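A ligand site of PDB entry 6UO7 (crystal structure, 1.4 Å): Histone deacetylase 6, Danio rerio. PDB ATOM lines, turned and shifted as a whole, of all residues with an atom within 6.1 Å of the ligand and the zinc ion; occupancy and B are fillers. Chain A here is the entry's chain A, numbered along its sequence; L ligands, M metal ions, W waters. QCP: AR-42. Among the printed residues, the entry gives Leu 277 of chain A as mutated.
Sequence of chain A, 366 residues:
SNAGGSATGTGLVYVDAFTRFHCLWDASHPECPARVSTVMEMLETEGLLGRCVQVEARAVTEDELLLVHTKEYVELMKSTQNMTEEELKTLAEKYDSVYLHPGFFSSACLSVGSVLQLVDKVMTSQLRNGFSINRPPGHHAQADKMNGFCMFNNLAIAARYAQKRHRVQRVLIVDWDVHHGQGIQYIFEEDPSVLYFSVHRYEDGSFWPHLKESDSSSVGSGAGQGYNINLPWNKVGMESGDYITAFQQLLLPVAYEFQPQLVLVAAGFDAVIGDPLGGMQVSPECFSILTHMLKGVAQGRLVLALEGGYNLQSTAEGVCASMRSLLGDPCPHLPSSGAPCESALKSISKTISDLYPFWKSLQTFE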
ATOM      1  N   ASP A  26      25.007  12.839  24.504  1.00  0.00           N
ATOM      2  CA  ASP A  26      26.097  12.467  23.609  1.00  0.00           C
ATOM      3  C   ASP A  26      25.585  12.582  22.173  1.00  0.00           C
ATOM      4  O   ASP A  26      24.957  11.653  21.664  1.00  0.00           O
ATOM      5  CB  ASP A  26      26.611  11.066  23.899  1.00  0.00           C
ATOM      6  CG  ASP A  26      27.696  10.624  22.926  1.00  0.00           C
ATOM      7  OD1 ASP A  26      28.168  11.453  22.124  1.00  0.00           O
ATOM      8  OD2 ASP A  26      28.090   9.436  22.969  1.00  0.00           O
ATOM      9  N   SER A  28      27.114  12.343  19.486  1.00  0.00           N
ATOM     10  CA  SER A  28      27.758  11.397  18.574  1.00  0.00           C
ATOM     11  C   SER A  28      27.372   9.954  18.841  1.00  0.00           C
ATOM     12  O   SER A  28      27.977   9.042  18.274  1.00  0.00           O
ATOM     13  CB  SER A  28      29.276  11.546  18.633  1.00  0.00           C
ATOM     14  OG  SER A  28      29.678  12.859  18.272  1.00  0.00           O
ATOM     15  N   HIS A  29      26.394   9.719  19.710  1.00  0.00           N
ATOM     16  CA  HIS A  29      26.023   8.350  20.035  1.00  0.00           C
ATOM     17  C   HIS A  29      25.635   7.606  18.770  1.00  0.00           C
ATOM     18  O   HIS A  29      24.877   8.138  17.945  1.00  0.00           O
ATOM     19  CB  HIS A  29      24.859   8.319  21.021  1.00  0.00           C
ATOM     20  CG  HIS A  29      24.696   6.982  21.694  1.00  0.00           C
ATOM     21  ND1 HIS A  29      24.212   5.872  21.030  1.00  0.00           N
ATOM     22  CD2 HIS A  29      24.976   6.586  22.951  1.00  0.00           C
ATOM     23  CE1 HIS A  29      24.202   4.846  21.862  1.00  0.00           C
ATOM     24  NE2 HIS A  29      24.655   5.254  23.032  1.00  0.00           N
ATOM     25  N   PRO A  30      26.123   6.379  18.566  1.00  0.00           N
ATOM     26  CA  PRO A  30      25.865   5.686  17.298  1.00  0.00           C
ATOM     27  C   PRO A  30      24.424   5.226  17.126  1.00  0.00           C
ATOM     28  O   PRO A  30      23.976   5.060  15.986  1.00  0.00           O
ATOM     29  CB  PRO A  30      26.832   4.499  17.347  1.00  0.00           C
ATOM     30  CG  PRO A  30      27.042   4.245  18.806  1.00  0.00           C
ATOM     31  CD  PRO A  30      27.068   5.628  19.421  1.00  0.00           C
ATOM     32  N   SER A  97      26.165   0.233  29.012  1.00  0.00           N
ATOM     33  CA  SER A  97      26.069   0.699  27.625  1.00  0.00           C
ATOM     34  C   SER A  97      24.624   0.977  27.202  1.00  0.00           C
ATOM     35  O   SER A  97      24.143   0.452  26.199  1.00  0.00           O
ATOM     36  CB  SER A  97      26.759  -0.286  26.678  1.00  0.00           C
ATOM     37  OG  SER A  97      26.697   0.212  25.347  1.00  0.00           O
ATOM     38  N   VAL A  98      23.933   1.835  27.954  1.00  0.00           N
ATOM     39  CA  VAL A  98      22.616   2.316  27.557  1.00  0.00           C
ATOM     40  C   VAL A  98      22.493   3.800  27.836  1.00  0.00           C
ATOM     41  O   VAL A  98      23.163   4.355  28.719  1.00  0.00           O
ATOM     42  CB  VAL A  98      21.439   1.577  28.245  1.00  0.00           C
ATOM     43  CG1 VAL A  98      21.568   0.082  28.070  1.00  0.00           C
ATOM     44  CG2 VAL A  98      21.367   1.929  29.711  1.00  0.00           C
ATOM     45  N   PRO A 137      16.820  -1.465  19.559  1.00  0.00           N
ATOM     46  CA  PRO A 137      17.103  -2.894  19.376  1.00  0.00           C
ATOM     47  C   PRO A 137      16.752  -3.667  20.639  1.00  0.00           C
ATOM     48  O   PRO A 137      16.399  -3.084  21.675  1.00  0.00           O
ATOM     49  CB  PRO A 137      18.607  -2.895  19.115  1.00  0.00           C
ATOM     50  CG  PRO A 137      19.114  -1.736  19.915  1.00  0.00           C
ATOM     51  CD  PRO A 137      18.046  -0.675  19.689  1.00  0.00           C
ATOM     52  N   HIS A 139      18.265  -7.417  21.400  1.00  0.00           N
ATOM     53  CA  HIS A 139      18.823  -8.733  21.719  1.00  0.00           C
ATOM     54  C   HIS A 139      19.671  -8.769  22.990  1.00  0.00           C
ATOM     55  O   HIS A 139      19.921  -9.867  23.514  1.00  0.00           O
ATOM     56  CB  HIS A 139      19.515  -9.403  20.523  1.00  0.00           C
ATOM     57  CG  HIS A 139      20.757  -8.724  20.048  1.00  0.00           C
ATOM     58  ND1 HIS A 139      21.768  -9.422  19.422  1.00  0.00           N
ATOM     59  CD2 HIS A 139      21.152  -7.423  20.077  1.00  0.00           C
ATOM     60  CE1 HIS A 139      22.738  -8.590  19.105  1.00  0.00           C
ATOM     61  NE2 HIS A 139      22.383  -7.360  19.472  1.00  0.00           N
ATOM     62  N   HIS A 140      20.138  -7.627  23.487  1.00  0.00           N
ATOM     63  CA  HIS A 140      20.882  -7.603  24.750  1.00  0.00           C
ATOM     64  C   HIS A 140      19.996  -7.436  25.980  1.00  0.00           C
ATOM     65  O   HIS A 140      20.482  -7.660  27.093  1.00  0.00           O
ATOM     66  CB  HIS A 140      21.890  -6.458  24.754  1.00  0.00           C
ATOM     67  CG  HIS A 140      22.914  -6.559  23.673  1.00  0.00           C
ATOM     68  ND1 HIS A 140      23.757  -7.642  23.543  1.00  0.00           N
ATOM     69  CD2 HIS A 140      23.218  -5.728  22.649  1.00  0.00           C
ATOM     70  CE1 HIS A 140      24.537  -7.470  22.500  1.00  0.00           C
ATOM     71  NE2 HIS A 140      24.237  -6.313  21.941  1.00  0.00           N
ATOM     72  N   GLY A 148      23.208  -2.669  26.491  1.00  0.00           N
ATOM     73  CA  GLY A 148      23.627  -2.614  25.094  1.00  0.00           C
ATOM     74  C   GLY A 148      22.638  -1.952  24.162  1.00  0.00           C
ATOM     75  O   GLY A 148      22.316  -2.490  23.087  1.00  0.00           O
ATOM     76  N   PHE A 149      22.127  -0.789  24.567  1.00  0.00           N
ATOM     77  CA  PHE A 149      21.218   0.052  23.796  1.00  0.00           C
ATOM     78  C   PHE A 149      19.798  -0.503  23.769  1.00  0.00           C
ATOM     79  O   PHE A 149      18.953   0.035  23.043  1.00  0.00           O
ATOM     80  CB  PHE A 149      21.662   0.317  22.346  1.00  0.00           C
ATOM     81  CG  PHE A 149      23.073   0.835  22.192  1.00  0.00           C
ATOM     82  CD1 PHE A 149      23.742   0.670  20.981  1.00  0.00           C
ATOM     83  CD2 PHE A 149      23.749   1.471  23.233  1.00  0.00           C
ATOM     84  CE1 PHE A 149      25.032   1.137  20.793  1.00  0.00           C
ATOM     85  CE2 PHE A 149      25.053   1.937  23.062  1.00  0.00           C
ATOM     86  CZ  PHE A 149      25.697   1.765  21.837  1.00  0.00           C
ATOM     87  N   CYS A 150      19.510  -1.551  24.547  1.00  0.00           N
ATOM     88  CA  CYS A 150      18.248  -2.277  24.493  1.00  0.00           C
ATOM     89  C   CYS A 150      17.502  -2.151  25.819  1.00  0.00           C
ATOM     90  O   CYS A 150      18.103  -2.241  26.887  1.00  0.00           O
ATOM     91  CB  CYS A 150      18.470  -3.775  24.259  1.00  0.00           C
ATOM     92  SG  CYS A 150      19.376  -4.186  22.761  1.00  0.00           S
ATOM     93  N   ASP A 177      23.740 -10.180  13.976  1.00  0.00           N
ATOM     94  CA  ASP A 177      24.373  -8.977  14.466  1.00  0.00           C
ATOM     95  C   ASP A 177      25.805  -9.317  14.911  1.00  0.00           C
ATOM     96  O   ASP A 177      26.086 -10.443  15.333  1.00  0.00           O
ATOM     97  CB  ASP A 177      23.537  -8.459  15.643  1.00  0.00           C
ATOM     98  CG  ASP A 177      24.003  -7.124  16.153  1.00  0.00           C
ATOM     99  OD1 ASP A 177      25.015  -7.053  16.899  1.00  0.00           O
ATOM    100  OD2 ASP A 177      23.353  -6.105  15.828  1.00  0.00           O
ATOM    101  N   VAL A 178      26.709  -8.348  14.803  1.00  0.00           N
ATOM    102  CA  VAL A 178      28.111  -8.611  15.124  1.00  0.00           C
ATOM    103  C   VAL A 178      28.340  -8.854  16.621  1.00  0.00           C
ATOM    104  O   VAL A 178      29.396  -9.368  17.001  1.00  0.00           O
ATOM    105  CB  VAL A 178      29.022  -7.477  14.596  1.00  0.00           C
ATOM    106  CG1 VAL A 178      29.052  -6.294  15.569  1.00  0.00           C
ATOM    107  CG2 VAL A 178      30.429  -7.998  14.312  1.00  0.00           C
ATOM    108  N   HIS A 179      27.385  -8.480  17.459  1.00  0.00           N
ATOM    109  CA  HIS A 179      27.491  -8.692  18.897  1.00  0.00           C
ATOM    110  C   HIS A 179      26.720  -9.940  19.307  1.00  0.00           C
ATOM    111  O   HIS A 179      25.740 -10.331  18.678  1.00  0.00           O
ATOM    112  CB  HIS A 179      26.904  -7.493  19.649  1.00  0.00           C
ATOM    113  CG  HIS A 179      27.619  -6.216  19.389  1.00  0.00           C
ATOM    114  ND1 HIS A 179      27.217  -5.311  18.427  1.00  0.00           N
ATOM    115  CD2 HIS A 179      28.720  -5.678  19.964  1.00  0.00           C
ATOM    116  CE1 HIS A 179      28.038  -4.277  18.417  1.00  0.00           C
ATOM    117  NE2 HIS A 179      28.954  -4.475  19.342  1.00  0.00           N
ATOM    118  N   TRP A 208      33.328  -6.165  23.220  1.00  0.00           N
ATOM    119  CA  TRP A 208      32.123  -6.045  24.029  1.00  0.00           C
ATOM    120  C   TRP A 208      31.072  -7.071  23.564  1.00  0.00           C
ATOM    121  O   TRP A 208      30.908  -7.266  22.348  1.00  0.00           O
ATOM    122  CB  TRP A 208      31.578  -4.613  23.888  1.00  0.00           C
ATOM    123  CG  TRP A 208      30.510  -4.303  24.880  1.00  0.00           C
ATOM    124  CD1 TRP A 208      30.669  -3.699  26.099  1.00  0.00           C
ATOM    125  CD2 TRP A 208      29.111  -4.593  24.759  1.00  0.00           C
ATOM    126  NE1 TRP A 208      29.456  -3.598  26.740  1.00  0.00           N
ATOM    127  CE2 TRP A 208      28.479  -4.138  25.938  1.00  0.00           C
ATOM    128  CE3 TRP A 208      28.320  -5.187  23.762  1.00  0.00           C
ATOM    129  CZ2 TRP A 208      27.111  -4.271  26.158  1.00  0.00           C
ATOM    130  CZ3 TRP A 208      26.965  -5.326  23.982  1.00  0.00           C
ATOM    131  CH2 TRP A 208      26.375  -4.880  25.167  1.00  0.00           C
ATOM    132  N   HIS A 210      32.276  -8.856  26.266  1.00  0.00           N
ATOM    133  CA  HIS A 210      33.394  -9.398  27.059  1.00  0.00           C
ATOM    134  C   HIS A 210      33.012 -10.578  27.941  1.00  0.00           C
ATOM    135  O   HIS A 210      33.563 -10.709  29.045  1.00  0.00           O
ATOM    136  CB  HIS A 210      34.011  -8.313  27.954  1.00  0.00           C
ATOM    137  CG  HIS A 210      34.250  -7.002  27.264  1.00  0.00           C
ATOM    138  ND1 HIS A 210      35.204  -6.830  26.293  1.00  0.00           N
ATOM    139  CD2 HIS A 210      33.670  -5.792  27.435  1.00  0.00           C
ATOM    140  CE1 HIS A 210      35.196  -5.576  25.877  1.00  0.00           C
ATOM    141  NE2 HIS A 210      34.272  -4.919  26.567  1.00  0.00           N
ATOM    142  N   GLY A 268      20.895  -7.475  12.773  1.00  0.00           N
ATOM    143  CA  GLY A 268      21.808  -6.363  12.868  1.00  0.00           C
ATOM    144  C   GLY A 268      22.712  -6.312  11.656  1.00  0.00           C
ATOM    145  O   GLY A 268      22.951  -7.323  11.000  1.00  0.00           O
ATOM    146  N   ASP A 270      25.828  -4.498  11.777  1.00  0.00           N
ATOM    147  CA  ASP A 270      27.117  -3.988  12.203  1.00  0.00           C
ATOM    148  C   ASP A 270      28.281  -4.879  11.798  1.00  0.00           C
ATOM    149  O   ASP A 270      29.430  -4.497  12.032  1.00  0.00           O
ATOM    150  CB  ASP A 270      27.135  -3.605  13.698  1.00  0.00           C
ATOM    151  CG  ASP A 270      26.385  -4.585  14.584  1.00  0.00           C
ATOM    152  OD1 ASP A 270      26.076  -5.698  14.135  1.00  0.00           O
ATOM    153  OD2 ASP A 270      26.096  -4.212  15.750  1.00  0.00           O
ATOM    154  N   LEU A 277      32.013   0.243  14.250  1.00  0.00           N
ATOM    155  CA  LEU A 277      32.288  -0.538  15.458  1.00  0.00           C
ATOM    156  C   LEU A 277      32.532  -2.025  15.202  1.00  0.00           C
ATOM    157  O   LEU A 277      33.261  -2.664  15.954  1.00  0.00           O
ATOM    158  CB  LEU A 277      31.073  -0.497  16.405  1.00  0.00           C
ATOM    159  CG  LEU A 277      30.509   0.845  16.853  1.00  0.00           C
ATOM    160  CD1 LEU A 277      29.275   0.661  17.719  1.00  0.00           C
ATOM    161  CD2 LEU A 277      31.577   1.621  17.586  1.00  0.00           C
ATOM    162  N   GLU A 307      18.384  -4.990  14.608  1.00  0.00           N
ATOM    163  CA  GLU A 307      19.135  -4.881  15.856  1.00  0.00           C
ATOM    164  C   GLU A 307      20.123  -3.730  15.675  1.00  0.00           C
ATOM    165  O   GLU A 307      19.689  -2.587  15.556  1.00  0.00           O
ATOM    166  CB  GLU A 307      19.786  -6.225  16.230  1.00  0.00           C
ATOM    167  CG  GLU A 307      18.764  -7.338  16.493  1.00  0.00           C
ATOM    168  CD  GLU A 307      18.056  -7.249  17.837  1.00  0.00           C
ATOM    169  OE1 GLU A 307      17.158  -8.086  18.066  1.00  0.00           O
ATOM    170  OE2 GLU A 307      18.373  -6.360  18.667  1.00  0.00           O
ATOM    171  N   GLY A 308      21.430  -4.017  15.627  1.00  0.00           N
ATOM    172  CA  GLY A 308      22.433  -2.989  15.445  1.00  0.00           C
ATOM    173  C   GLY A 308      22.752  -2.712  13.983  1.00  0.00           C
ATOM    174  O   GLY A 308      22.047  -3.105  13.057  1.00  0.00           O
ATOM    175  N   GLY A 309      23.861  -1.989  13.786  1.00  0.00           N
ATOM    176  CA  GLY A 309      24.272  -1.504  12.482  1.00  0.00           C
ATOM    177  C   GLY A 309      24.316   0.000  12.519  1.00  0.00           C
ATOM    178  O   GLY A 309      23.272   0.647  12.666  1.00  0.00           O
ATOM    179  N   TYR A 310      25.511   0.588  12.361  1.00  0.00           N
ATOM    180  CA  TYR A 310      25.735   1.989  12.709  1.00  0.00           C
ATOM    181  C   TYR A 310      26.322   2.841  11.603  1.00  0.00           C
ATOM    182  O   TYR A 310      26.421   4.063  11.782  1.00  0.00           O
ATOM    183  CB  TYR A 310      26.581   2.088  13.995  1.00  0.00           C
ATOM    184  CG  TYR A 310      25.885   1.324  15.087  1.00  0.00           C
ATOM    185  CD1 TYR A 310      24.736   1.828  15.674  1.00  0.00           C
ATOM    186  CD2 TYR A 310      26.289   0.048  15.437  1.00  0.00           C
ATOM    187  CE1 TYR A 310      24.026   1.104  16.632  1.00  0.00           C
ATOM    188  CE2 TYR A 310      25.598  -0.687  16.372  1.00  0.00           C
ATOM    189  CZ  TYR A 310      24.480  -0.145  16.978  1.00  0.00           C
ATOM    190  OH  TYR A 310      23.785  -0.871  17.924  1.00  0.00           O
HETATM  191  C10 QCP L   1      31.489   0.989  24.101  1.00  0.00           C
HETATM  192  C13 QCP L   1      29.488   2.494  23.511  1.00  0.00           C
HETATM  193  C15 QCP L   1      29.418   4.368  21.942  1.00  0.00           C
HETATM  194  C17 QCP L   1      28.126   4.464  23.934  1.00  0.00           C
HETATM  195  C20 QCP L   1      27.532  -1.036  20.758  1.00  0.00           C
HETATM  196  C21 QCP L   1      26.743  -1.754  19.886  1.00  0.00           C
HETATM  197  C02 QCP L   1      25.060  -3.461  19.376  1.00  0.00           C
HETATM  198  C03 QCP L   1      25.809  -2.669  20.334  1.00  0.00           C
HETATM  199  C04 QCP L   1      25.737  -2.832  21.723  1.00  0.00           C
HETATM  200  C05 QCP L   1      26.530  -2.105  22.598  1.00  0.00           C
HETATM  201  C06 QCP L   1      27.469  -1.196  22.158  1.00  0.00           C
HETATM  202  C08 QCP L   1      29.462   0.160  22.828  1.00  0.00           C
HETATM  203  C09 QCP L   1      29.985   1.084  23.893  1.00  0.00           C
HETATM  204  C11 QCP L   1      31.909  -0.416  24.546  1.00  0.00           C
HETATM  205  C12 QCP L   1      31.986   1.974  25.158  1.00  0.00           C
HETATM  206  C14 QCP L   1      29.872   3.105  22.321  1.00  0.00           C
HETATM  207  C16 QCP L   1      28.542   5.058  22.752  1.00  0.00           C
HETATM  208  C18 QCP L   1      28.584   3.206  24.300  1.00  0.00           C
HETATM  209  N07 QCP L   1      28.210  -0.436  22.980  1.00  0.00           N
HETATM  210  N22 QCP L   1      24.580  -4.718  19.795  1.00  0.00           N
HETATM  211  O01 QCP L   1      24.951  -3.177  18.213  1.00  0.00           O
HETATM  212  O19 QCP L   1      30.110  -0.052  21.803  1.00  0.00           O
HETATM  213  O23 QCP L   1      23.924  -5.535  18.939  1.00  0.00           O
HETATM  214 ZN    ZN M   1      25.331  -5.129  17.407  1.00  0.00          ZN
HETATM  215  O   HOH W   1      30.513   4.844  18.716  1.00  0.00           O
HETATM  216  O   HOH W   2      32.582   0.680  20.804  1.00  0.00           O
HETATM  217  O   HOH W   3      30.737  -2.530  20.317  1.00  0.00           O
HETATM  218  O   HOH W   4      27.349   4.052  27.434  1.00  0.00           O
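The zinc ion is bound by OD1 of Asp 177 (2.0 Å).
OD2 of Asp 270 is bound to the zinc ion.
The zinc ion is bound by O23 of the ligand (2.1 Å).
An oxygen (O01) of the ligand binds the zinc ion, 2.1 Å away.
The zinc ion is bound by a ring nitrogen (ND1) of His 179 (2.2 Å).
Slightly farther from the zinc ion lies OD2 of Asp 177 (2.7 Å).
A ring nitrogen (NE2) of His 139 sits close to an oxygen (O23) of the ligand.
The side-chain hydroxyl (OH) of Tyr 310 lies close to an oxygen (O01) of the ligand.
A nitrogen (N22) of the ligand sits close to a ring nitrogen (NE2) of His 140, 2.7 Å away.
N07 of the ligand sits at hydrogen-bond distance from OG of Ser 97 (2.9 Å).
Water W3 lies within hydrogen-bond range of NE2 of His 179 (2.8 Å) and O19 of the ligand (3.0 Å).
N of Gly 308 sits at hydrogen-bond distance from OD2 of Asp 177 (2.8 Å).
N of Val 178 is in hydrogen-bond range of OD1 of Asp 270 (2.8 Å).
The side-chain carboxylate (OE2) of Glu 307 is in hydrogen-bond range of the backbone NH (N) of His 139 (2.9 Å).
The side-chain sulfur of Cys 150 sits at hydrogen-bond distance from the backbone NH of His 139 (3.7 Å).
The side-chain sulfur (SG) of Cys 150 sits at hydrogen-bond distance from the backbone NH (N) of His 140 (3.6 Å).
The backbone carbonyl oxygen of Ser 97 sits at hydrogen-bond distance from the backbone NH of Phe 149, at 2.9 Å.
O of Ser 97 lies within hydrogen-bond range of N of Gly 148.
O of Gly 148 sits at hydrogen-bond distance from SG of Cys 150, at 3.4 Å.
His 29 touches the ligand.
Pro 30 touches the ligand (CD to C15, 3.7 Å).
Gly 148 touches the ligand.
CE1 of Phe 149 touches C20 of the ligand, 3.3 Å away.
Trp 208 touches the ligand (CZ3 to C05, 3.5 Å).
Leu 277 touches the ligand.
Gly 308 touches the ligand.
Hydrophobic or aromatic side chains within 4 Å of the ligand: His 29, Pro 30, His 139, His 140, Phe 149, His 179, Trp 208, Leu 277 and Tyr 310.
Within 4 Å of the ligand: His 29, Pro 30, Ser 97, His 139, His 140, Gly 148, Phe 149, Asp 177, His 179, Trp 208, Asp 270, Leu 277, Gly 308 and Tyr 310.
Within 4 Å of the zinc ion: Asp 177, His 179 and Asp 270.
Along chain A the residues within 4 Å of the zinc ion span positions 177 to 270.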
